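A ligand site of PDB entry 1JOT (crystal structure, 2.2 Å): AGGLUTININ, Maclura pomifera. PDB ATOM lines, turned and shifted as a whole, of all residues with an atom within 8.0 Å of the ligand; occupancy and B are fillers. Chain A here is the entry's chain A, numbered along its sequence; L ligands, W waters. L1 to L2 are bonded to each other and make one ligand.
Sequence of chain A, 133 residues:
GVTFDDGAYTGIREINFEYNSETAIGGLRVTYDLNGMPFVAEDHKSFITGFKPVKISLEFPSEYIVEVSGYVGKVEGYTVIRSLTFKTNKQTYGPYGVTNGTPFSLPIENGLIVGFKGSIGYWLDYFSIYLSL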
ATOM      1  N   GLY A   1     -12.121   0.314 -25.508  1.00  0.00           N
ATOM      2  CA  GLY A   1     -12.616  -0.007 -24.133  1.00  0.00           C
ATOM      3  C   GLY A   1     -13.598  -1.167 -24.138  1.00  0.00           C
ATOM      4  O   GLY A   1     -13.867  -1.742 -25.180  1.00  0.00           O
ATOM      5  N   VAL A   2     -14.116  -1.498 -22.967  1.00  0.00           N
ATOM      6  CA  VAL A   2     -15.084  -2.584 -22.843  1.00  0.00           C
ATOM      7  C   VAL A   2     -16.478  -1.985 -22.939  1.00  0.00           C
ATOM      8  O   VAL A   2     -16.839  -1.079 -22.181  1.00  0.00           O
ATOM      9  CB  VAL A   2     -14.922  -3.316 -21.486  1.00  0.00           C
ATOM     10  CG1 VAL A   2     -16.105  -4.236 -21.218  1.00  0.00           C
ATOM     11  CG2 VAL A   2     -13.641  -4.124 -21.506  1.00  0.00           C
ATOM     12  N   THR A   3     -17.264  -2.470 -23.881  1.00  0.00           N
ATOM     13  CA  THR A   3     -18.602  -1.944 -24.056  1.00  0.00           C
ATOM     14  C   THR A   3     -19.551  -2.457 -22.972  1.00  0.00           C
ATOM     15  O   THR A   3     -19.369  -3.547 -22.417  1.00  0.00           O
ATOM     16  CB  THR A   3     -19.162  -2.315 -25.428  1.00  0.00           C
ATOM     17  OG1 THR A   3     -19.332  -3.732 -25.491  1.00  0.00           O
ATOM     18  CG2 THR A   3     -18.205  -1.866 -26.522  1.00  0.00           C
ATOM     19  N   ALA A  24      -9.899  13.030 -18.315  1.00  0.00           N
ATOM     20  CA  ALA A  24     -11.284  12.875 -18.755  1.00  0.00           C
ATOM     21  C   ALA A  24     -12.129  12.104 -17.761  1.00  0.00           C
ATOM     22  O   ALA A  24     -11.733  11.874 -16.614  1.00  0.00           O
ATOM     23  CB  ALA A  24     -11.288  12.153 -20.104  1.00  0.00           C
ATOM     24  N   ILE A  25     -13.313  11.694 -18.216  1.00  0.00           N
ATOM     25  CA  ILE A  25     -14.230  10.939 -17.373  1.00  0.00           C
ATOM     26  C   ILE A  25     -13.779   9.475 -17.307  1.00  0.00           C
ATOM     27  O   ILE A  25     -13.355   8.888 -18.316  1.00  0.00           O
ATOM     28  CB  ILE A  25     -15.680  11.018 -17.910  1.00  0.00           C
ATOM     29  CG1 ILE A  25     -16.165  12.474 -17.915  1.00  0.00           C
ATOM     30  CG2 ILE A  25     -16.610  10.148 -17.057  1.00  0.00           C
ATOM     31  CD1 ILE A  25     -16.340  13.089 -16.533  1.00  0.00           C
ATOM     32  N   SER A  46     -12.800   1.991 -14.998  1.00  0.00           N
ATOM     33  CA  SER A  46     -11.738   2.465 -15.862  1.00  0.00           C
ATOM     34  C   SER A  46     -10.610   1.438 -15.808  1.00  0.00           C
ATOM     35  O   SER A  46     -10.505   0.689 -14.836  1.00  0.00           O
ATOM     36  CB  SER A  46     -11.230   3.810 -15.334  1.00  0.00           C
ATOM     37  OG  SER A  46      -9.973   4.140 -15.871  1.00  0.00           O
ATOM     38  N   PHE A  47      -9.761   1.408 -16.834  1.00  0.00           N
ATOM     39  CA  PHE A  47      -8.647   0.467 -16.864  1.00  0.00           C
ATOM     40  C   PHE A  47      -7.537   0.955 -15.931  1.00  0.00           C
ATOM     41  O   PHE A  47      -6.598   0.210 -15.652  1.00  0.00           O
ATOM     42  CB  PHE A  47      -8.055   0.349 -18.272  1.00  0.00           C
ATOM     43  CG  PHE A  47      -8.901  -0.446 -19.229  1.00  0.00           C
ATOM     44  CD1 PHE A  47     -10.128  -0.966 -18.851  1.00  0.00           C
ATOM     45  CD2 PHE A  47      -8.480  -0.638 -20.544  1.00  0.00           C
ATOM     46  CE1 PHE A  47     -10.923  -1.669 -19.763  1.00  0.00           C
ATOM     47  CE2 PHE A  47      -9.258  -1.346 -21.456  1.00  0.00           C
ATOM     48  CZ  PHE A  47     -10.476  -1.859 -21.066  1.00  0.00           C
ATOM     49  N   ILE A  48      -7.628   2.195 -15.473  1.00  0.00           N
ATOM     50  CA  ILE A  48      -6.617   2.787 -14.596  1.00  0.00           C
ATOM     51  C   ILE A  48      -7.199   3.432 -13.349  1.00  0.00           C
ATOM     52  O   ILE A  48      -8.400   3.373 -13.094  1.00  0.00           O
ATOM     53  CB  ILE A  48      -5.800   3.847 -15.345  1.00  0.00           C
ATOM     54  CG1 ILE A  48      -6.734   4.859 -16.014  1.00  0.00           C
ATOM     55  CG2 ILE A  48      -4.907   3.187 -16.364  1.00  0.00           C
ATOM     56  CD1 ILE A  48      -6.020   6.010 -16.667  1.00  0.00           C
ATOM     57  N   VAL A  75      -7.511  12.597 -25.685  1.00  0.00           N
ATOM     58  CA  VAL A  75      -6.570  12.421 -24.579  1.00  0.00           C
ATOM     59  C   VAL A  75      -5.674  11.271 -25.007  1.00  0.00           C
ATOM     60  O   VAL A  75      -6.140  10.170 -25.300  1.00  0.00           O
ATOM     61  CB  VAL A  75      -7.277  12.073 -23.246  1.00  0.00           C
ATOM     62  CG1 VAL A  75      -6.239  11.687 -22.206  1.00  0.00           C
ATOM     63  CG2 VAL A  75      -8.076  13.260 -22.745  1.00  0.00           C
ATOM     64  N   GLU A  76      -4.369  11.532 -25.073  1.00  0.00           N
ATOM     65  CA  GLU A  76      -3.417  10.512 -25.487  1.00  0.00           C
ATOM     66  C   GLU A  76      -3.843   9.933 -26.835  1.00  0.00           C
ATOM     67  O   GLU A  76      -3.645   8.756 -27.108  1.00  0.00           O
ATOM     68  CB  GLU A  76      -3.323   9.403 -24.445  1.00  0.00           C
ATOM     69  CG  GLU A  76      -2.577   9.823 -23.180  1.00  0.00           C
ATOM     70  CD  GLU A  76      -1.065   9.947 -23.377  1.00  0.00           C
ATOM     71  OE1 GLU A  76      -0.553   9.629 -24.478  1.00  0.00           O
ATOM     72  OE2 GLU A  76      -0.377  10.367 -22.413  1.00  0.00           O
ATOM     73  N   GLY A  77      -4.465  10.782 -27.658  1.00  0.00           N
ATOM     74  CA  GLY A  77      -4.904  10.361 -28.980  1.00  0.00           C
ATOM     75  C   GLY A  77      -6.259   9.682 -29.070  1.00  0.00           C
ATOM     76  O   GLY A  77      -6.720   9.369 -30.171  1.00  0.00           O
ATOM     77  N   TYR A  78      -6.893   9.449 -27.931  1.00  0.00           N
ATOM     78  CA  TYR A  78      -8.189   8.797 -27.915  1.00  0.00           C
ATOM     79  C   TYR A  78      -9.289   9.829 -27.758  1.00  0.00           C
ATOM     80  O   TYR A  78      -9.142  10.781 -26.981  1.00  0.00           O
ATOM     81  CB  TYR A  78      -8.265   7.790 -26.749  1.00  0.00           C
ATOM     82  CG  TYR A  78      -7.449   6.536 -26.969  1.00  0.00           C
ATOM     83  CD1 TYR A  78      -7.805   5.605 -27.941  1.00  0.00           C
ATOM     84  CD2 TYR A  78      -6.307   6.290 -26.213  1.00  0.00           C
ATOM     85  CE1 TYR A  78      -7.037   4.466 -28.158  1.00  0.00           C
ATOM     86  CE2 TYR A  78      -5.537   5.152 -26.415  1.00  0.00           C
ATOM     87  CZ  TYR A  78      -5.915   4.248 -27.394  1.00  0.00           C
ATOM     88  OH  TYR A  78      -5.145   3.127 -27.598  1.00  0.00           O
ATOM     89  N   THR A  79     -10.383   9.662 -28.495  1.00  0.00           N
ATOM     90  CA  THR A  79     -11.516  10.589 -28.406  1.00  0.00           C
ATOM     91  C   THR A  79     -12.413  10.098 -27.286  1.00  0.00           C
ATOM     92  O   THR A  79     -13.014   9.030 -27.391  1.00  0.00           O
ATOM     93  CB  THR A  79     -12.326  10.616 -29.712  1.00  0.00           C
ATOM     94  OG1 THR A  79     -11.433  10.813 -30.817  1.00  0.00           O
ATOM     95  CG2 THR A  79     -13.354  11.745 -29.676  1.00  0.00           C
ATOM     96  N   VAL A  80     -12.508  10.878 -26.224  1.00  0.00           N
ATOM     97  CA  VAL A  80     -13.314  10.472 -25.076  1.00  0.00           C
ATOM     98  C   VAL A  80     -14.149  11.607 -24.490  1.00  0.00           C
ATOM     99  O   VAL A  80     -13.991  12.766 -24.862  1.00  0.00           O
ATOM    100  CB  VAL A  80     -12.392   9.920 -23.963  1.00  0.00           C
ATOM    101  CG1 VAL A  80     -11.505   8.807 -24.513  1.00  0.00           C
ATOM    102  CG2 VAL A  80     -11.518  11.035 -23.403  1.00  0.00           C
ATOM    103  N   ILE A  81     -15.040  11.251 -23.573  1.00  0.00           N
ATOM    104  CA  ILE A  81     -15.868  12.241 -22.912  1.00  0.00           C
ATOM    105  C   ILE A  81     -14.987  12.833 -21.815  1.00  0.00           C
ATOM    106  O   ILE A  81     -14.617  12.141 -20.873  1.00  0.00           O
ATOM    107  CB  ILE A  81     -17.104  11.583 -22.274  1.00  0.00           C
ATOM    108  CG1 ILE A  81     -17.840  10.755 -23.331  1.00  0.00           C
ATOM    109  CG2 ILE A  81     -18.011  12.636 -21.653  1.00  0.00           C
ATOM    110  CD1 ILE A  81     -18.697  11.560 -24.264  1.00  0.00           C
ATOM    111  N   SER A 119     -19.034   2.724 -23.700  1.00  0.00           N
ATOM    112  CA  SER A 119     -17.757   2.019 -23.656  1.00  0.00           C
ATOM    113  C   SER A 119     -16.758   2.743 -22.787  1.00  0.00           C
ATOM    114  O   SER A 119     -16.660   3.982 -22.832  1.00  0.00           O
ATOM    115  CB  SER A 119     -17.186   1.877 -25.068  1.00  0.00           C
ATOM    116  OG  SER A 119     -15.783   1.709 -25.019  1.00  0.00           O
ATOM    117  N   ILE A 120     -16.018   1.983 -21.983  1.00  0.00           N
ATOM    118  CA  ILE A 120     -14.997   2.546 -21.104  1.00  0.00           C
ATOM    119  C   ILE A 120     -13.701   1.741 -21.175  1.00  0.00           C
ATOM    120  O   ILE A 120     -13.717   0.519 -21.090  1.00  0.00           O
ATOM    121  CB  ILE A 120     -15.465   2.580 -19.630  1.00  0.00           C
ATOM    122  CG1 ILE A 120     -16.752   3.402 -19.496  1.00  0.00           C
ATOM    123  CG2 ILE A 120     -14.385   3.214 -18.755  1.00  0.00           C
ATOM    124  CD1 ILE A 120     -17.468   3.214 -18.181  1.00  0.00           C
ATOM    125  N   GLY A 121     -12.599   2.451 -21.355  1.00  0.00           N
ATOM    126  CA  GLY A 121     -11.275   1.834 -21.393  1.00  0.00           C
ATOM    127  C   GLY A 121     -10.541   2.545 -20.263  1.00  0.00           C
ATOM    128  O   GLY A 121     -10.806   2.279 -19.093  1.00  0.00           O
ATOM    129  N   TYR A 122      -9.645   3.462 -20.617  1.00  0.00           N
ATOM    130  CA  TYR A 122      -8.943   4.256 -19.618  1.00  0.00           C
ATOM    131  C   TYR A 122      -9.943   5.327 -19.189  1.00  0.00           C
ATOM    132  O   TYR A 122     -10.050   5.675 -18.008  1.00  0.00           O
ATOM    133  CB  TYR A 122      -7.713   4.927 -20.228  1.00  0.00           C
ATOM    134  CG  TYR A 122      -6.545   3.981 -20.426  1.00  0.00           C
ATOM    135  CD1 TYR A 122      -6.147   3.116 -19.417  1.00  0.00           C
ATOM    136  CD2 TYR A 122      -5.863   3.932 -21.649  1.00  0.00           C
ATOM    137  CE1 TYR A 122      -5.094   2.243 -19.595  1.00  0.00           C
ATOM    138  CE2 TYR A 122      -4.803   3.047 -21.841  1.00  0.00           C
ATOM    139  CZ  TYR A 122      -4.419   2.206 -20.804  1.00  0.00           C
ATOM    140  OH  TYR A 122      -3.380   1.323 -20.966  1.00  0.00           O
ATOM    141  N   TRP A 123     -10.687   5.819 -20.173  1.00  0.00           N
ATOM    142  CA  TRP A 123     -11.706   6.842 -19.938  1.00  0.00           C
ATOM    143  C   TRP A 123     -13.004   6.468 -20.640  1.00  0.00           C
ATOM    144  O   TRP A 123     -13.055   5.518 -21.426  1.00  0.00           O
ATOM    145  CB  TRP A 123     -11.196   8.193 -20.444  1.00  0.00           C
ATOM    146  CG  TRP A 123      -9.853   8.546 -19.887  1.00  0.00           C
ATOM    147  CD1 TRP A 123      -9.579   8.976 -18.613  1.00  0.00           C
ATOM    148  CD2 TRP A 123      -8.586   8.433 -20.555  1.00  0.00           C
ATOM    149  NE1 TRP A 123      -8.217   9.139 -18.450  1.00  0.00           N
ATOM    150  CE2 TRP A 123      -7.585   8.814 -19.625  1.00  0.00           C
ATOM    151  CE3 TRP A 123      -8.195   8.051 -21.846  1.00  0.00           C
ATOM    152  CZ2 TRP A 123      -6.213   8.815 -19.942  1.00  0.00           C
ATOM    153  CZ3 TRP A 123      -6.839   8.058 -22.162  1.00  0.00           C
ATOM    154  CH2 TRP A 123      -5.869   8.433 -21.215  1.00  0.00           C
ATOM    155  N   LEU A 124     -14.067   7.210 -20.337  1.00  0.00           N
ATOM    156  CA  LEU A 124     -15.367   6.969 -20.971  1.00  0.00           C
ATOM    157  C   LEU A 124     -15.199   7.267 -22.462  1.00  0.00           C
ATOM    158  O   LEU A 124     -14.965   8.403 -22.862  1.00  0.00           O
ATOM    159  CB  LEU A 124     -16.415   7.891 -20.348  1.00  0.00           C
ATOM    160  CG  LEU A 124     -17.862   7.778 -20.828  1.00  0.00           C
ATOM    161  CD1 LEU A 124     -18.403   6.393 -20.523  1.00  0.00           C
ATOM    162  CD2 LEU A 124     -18.711   8.832 -20.148  1.00  0.00           C
ATOM    163  N   ASP A 125     -15.301   6.225 -23.294  1.00  0.00           N
ATOM    164  CA  ASP A 125     -15.124   6.389 -24.719  1.00  0.00           C
ATOM    165  C   ASP A 125     -16.305   7.076 -25.384  1.00  0.00           C
ATOM    166  O   ASP A 125     -16.142   8.008 -26.181  1.00  0.00           O
ATOM    167  CB  ASP A 125     -14.898   5.029 -25.373  1.00  0.00           C
ATOM    168  CG  ASP A 125     -13.619   4.388 -24.914  1.00  0.00           C
ATOM    169  OD1 ASP A 125     -12.566   5.053 -24.979  1.00  0.00           O
ATOM    170  OD2 ASP A 125     -13.669   3.213 -24.486  1.00  0.00           O
ATOM    171  N   TYR A 126     -17.496   6.618 -25.043  1.00  0.00           N
ATOM    172  CA  TYR A 126     -18.716   7.178 -25.602  1.00  0.00           C
ATOM    173  C   TYR A 126     -19.895   6.563 -24.873  1.00  0.00           C
ATOM    174  O   TYR A 126     -19.758   5.519 -24.224  1.00  0.00           O
ATOM    175  CB  TYR A 126     -18.789   6.854 -27.095  1.00  0.00           C
ATOM    176  CG  TYR A 126     -18.732   5.386 -27.411  1.00  0.00           C
ATOM    177  CD1 TYR A 126     -19.845   4.563 -27.193  1.00  0.00           C
ATOM    178  CD2 TYR A 126     -17.573   4.803 -27.949  1.00  0.00           C
ATOM    179  CE1 TYR A 126     -19.806   3.204 -27.501  1.00  0.00           C
ATOM    180  CE2 TYR A 126     -17.526   3.451 -28.258  1.00  0.00           C
ATOM    181  CZ  TYR A 126     -18.643   2.651 -28.035  1.00  0.00           C
ATOM    182  OH  TYR A 126     -18.621   1.324 -28.379  1.00  0.00           O
HETATM  183  O1  LIG L   1      -8.480   3.099 -23.515  1.00  0.00           O
HETATM  184  C1  LIG L   1      -7.800   1.857 -23.830  1.00  0.00           C
HETATM  185  O2  LIG L   1      -6.572   2.174 -24.456  1.00  0.00           O
HETATM  186  C2  LIG L   1      -8.648   1.000 -24.774  1.00  0.00           C
HETATM  187  N1  LIG L   1      -7.915  -0.202 -25.125  1.00  0.00           N
HETATM  188  C3  LIG L   1      -8.995   1.796 -26.040  1.00  0.00           C
HETATM  189  O3  LIG L   1      -9.890   1.027 -26.858  1.00  0.00           O
HETATM  190  C4  LIG L   1      -9.669   3.112 -25.646  1.00  0.00           C
HETATM  191  O4  LIG L   1     -10.899   2.803 -24.999  1.00  0.00           O
HETATM  192  C5  LIG L   1      -8.760   3.892 -24.687  1.00  0.00           C
HETATM  193  C6  LIG L   1      -9.420   5.210 -24.274  1.00  0.00           C
HETATM  194  O5  LIG L   1     -10.200   5.010 -23.108  1.00  0.00           O
HETATM  195  C7  LIG L   1      -8.530  -1.386 -25.149  1.00  0.00           C
HETATM  196  O6  LIG L   1      -9.715  -1.531 -24.882  1.00  0.00           O
HETATM  197  C8  LIG L   1      -7.680  -2.597 -25.518  1.00  0.00           C
HETATM  198  C1  LG2 L   2      -9.441   0.909 -28.210  1.00  0.00           C
HETATM  199  C2  LG2 L   2     -10.090  -0.321 -28.854  1.00  0.00           C
HETATM  200  C3  LG2 L   2      -9.792  -0.420 -30.357  1.00  0.00           C
HETATM  201  C4  LG2 L   2     -10.070   0.907 -31.042  1.00  0.00           C
HETATM  202  C5  LG2 L   2      -9.318   2.028 -30.336  1.00  0.00           C
HETATM  203  C6  LG2 L   2      -9.566   3.359 -31.052  1.00  0.00           C
HETATM  204  O1  LG2 L   2      -9.594  -1.493 -28.209  1.00  0.00           O
HETATM  205  O2  LG2 L   2     -10.612  -1.424 -30.930  1.00  0.00           O
HETATM  206  O3  LG2 L   2     -11.467   1.168 -30.999  1.00  0.00           O
HETATM  207  O4  LG2 L   2      -9.760   2.108 -28.960  1.00  0.00           O
HETATM  208  O5  LG2 L   2      -9.345   4.437 -30.164  1.00  0.00           O
HETATM  209  O   HOH W   1     -10.860   7.084 -29.917  1.00  0.00           O
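An oxygen (O3) of LIG L1 sits at hydrogen-bond distance from the backbone NH of Gly 1 (2.7 Å).
The backbone NH (N) of Tyr 122 is in hydrogen-bond range of an oxygen (O5) of LIG L1 (3.0 Å).
The side-chain carboxylate (OD1) of Asp 125 sits at hydrogen-bond distance from an oxygen (O4) of LIG L1 (2.8 Å).
N of Trp 123 lies within hydrogen-bond range of O5 of LIG L1 (3.1 Å).
The backbone carbonyl oxygen (O) of Trp 123 sits at hydrogen-bond distance from an oxygen (O5) of LIG L1, at 3.4 Å.
The side-chain carboxylate (OD2) of Asp 125 lies close to the backbone NH (N) of Gly 1, 3.4 Å away.
The side-chain carboxylate of Asp 125 is in hydrogen-bond range of the backbone NH of Gly 121, 3.4 Å away.
The side-chain carboxylate (OD2) of Asp 125 sits at hydrogen-bond distance from the side-chain hydroxyl (OG) of Ser 119 (2.6 Å).
The side-chain hydroxyl of Ser 46 sits at hydrogen-bond distance from the backbone carbonyl oxygen of Tyr 122, 2.6 Å away.
O of Gly 121 sits at hydrogen-bond distance from N of Phe 47 (2.6 Å).
Residues that only touch the ligand: Tyr 78 (2.9 Å), Phe 47 (3.5 Å) and Gly 121 (3.7 Å).
Hydrophobic or aromatic side chains within 4 Å of the ligand: Phe 47, Tyr 78, Tyr 122 and Trp 123.
The nearest printed residue that does not touch the ligand is Val 80 (4.2 Å).
Water W1 bridges N of Thr 79 and O5 of LG2 L2.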
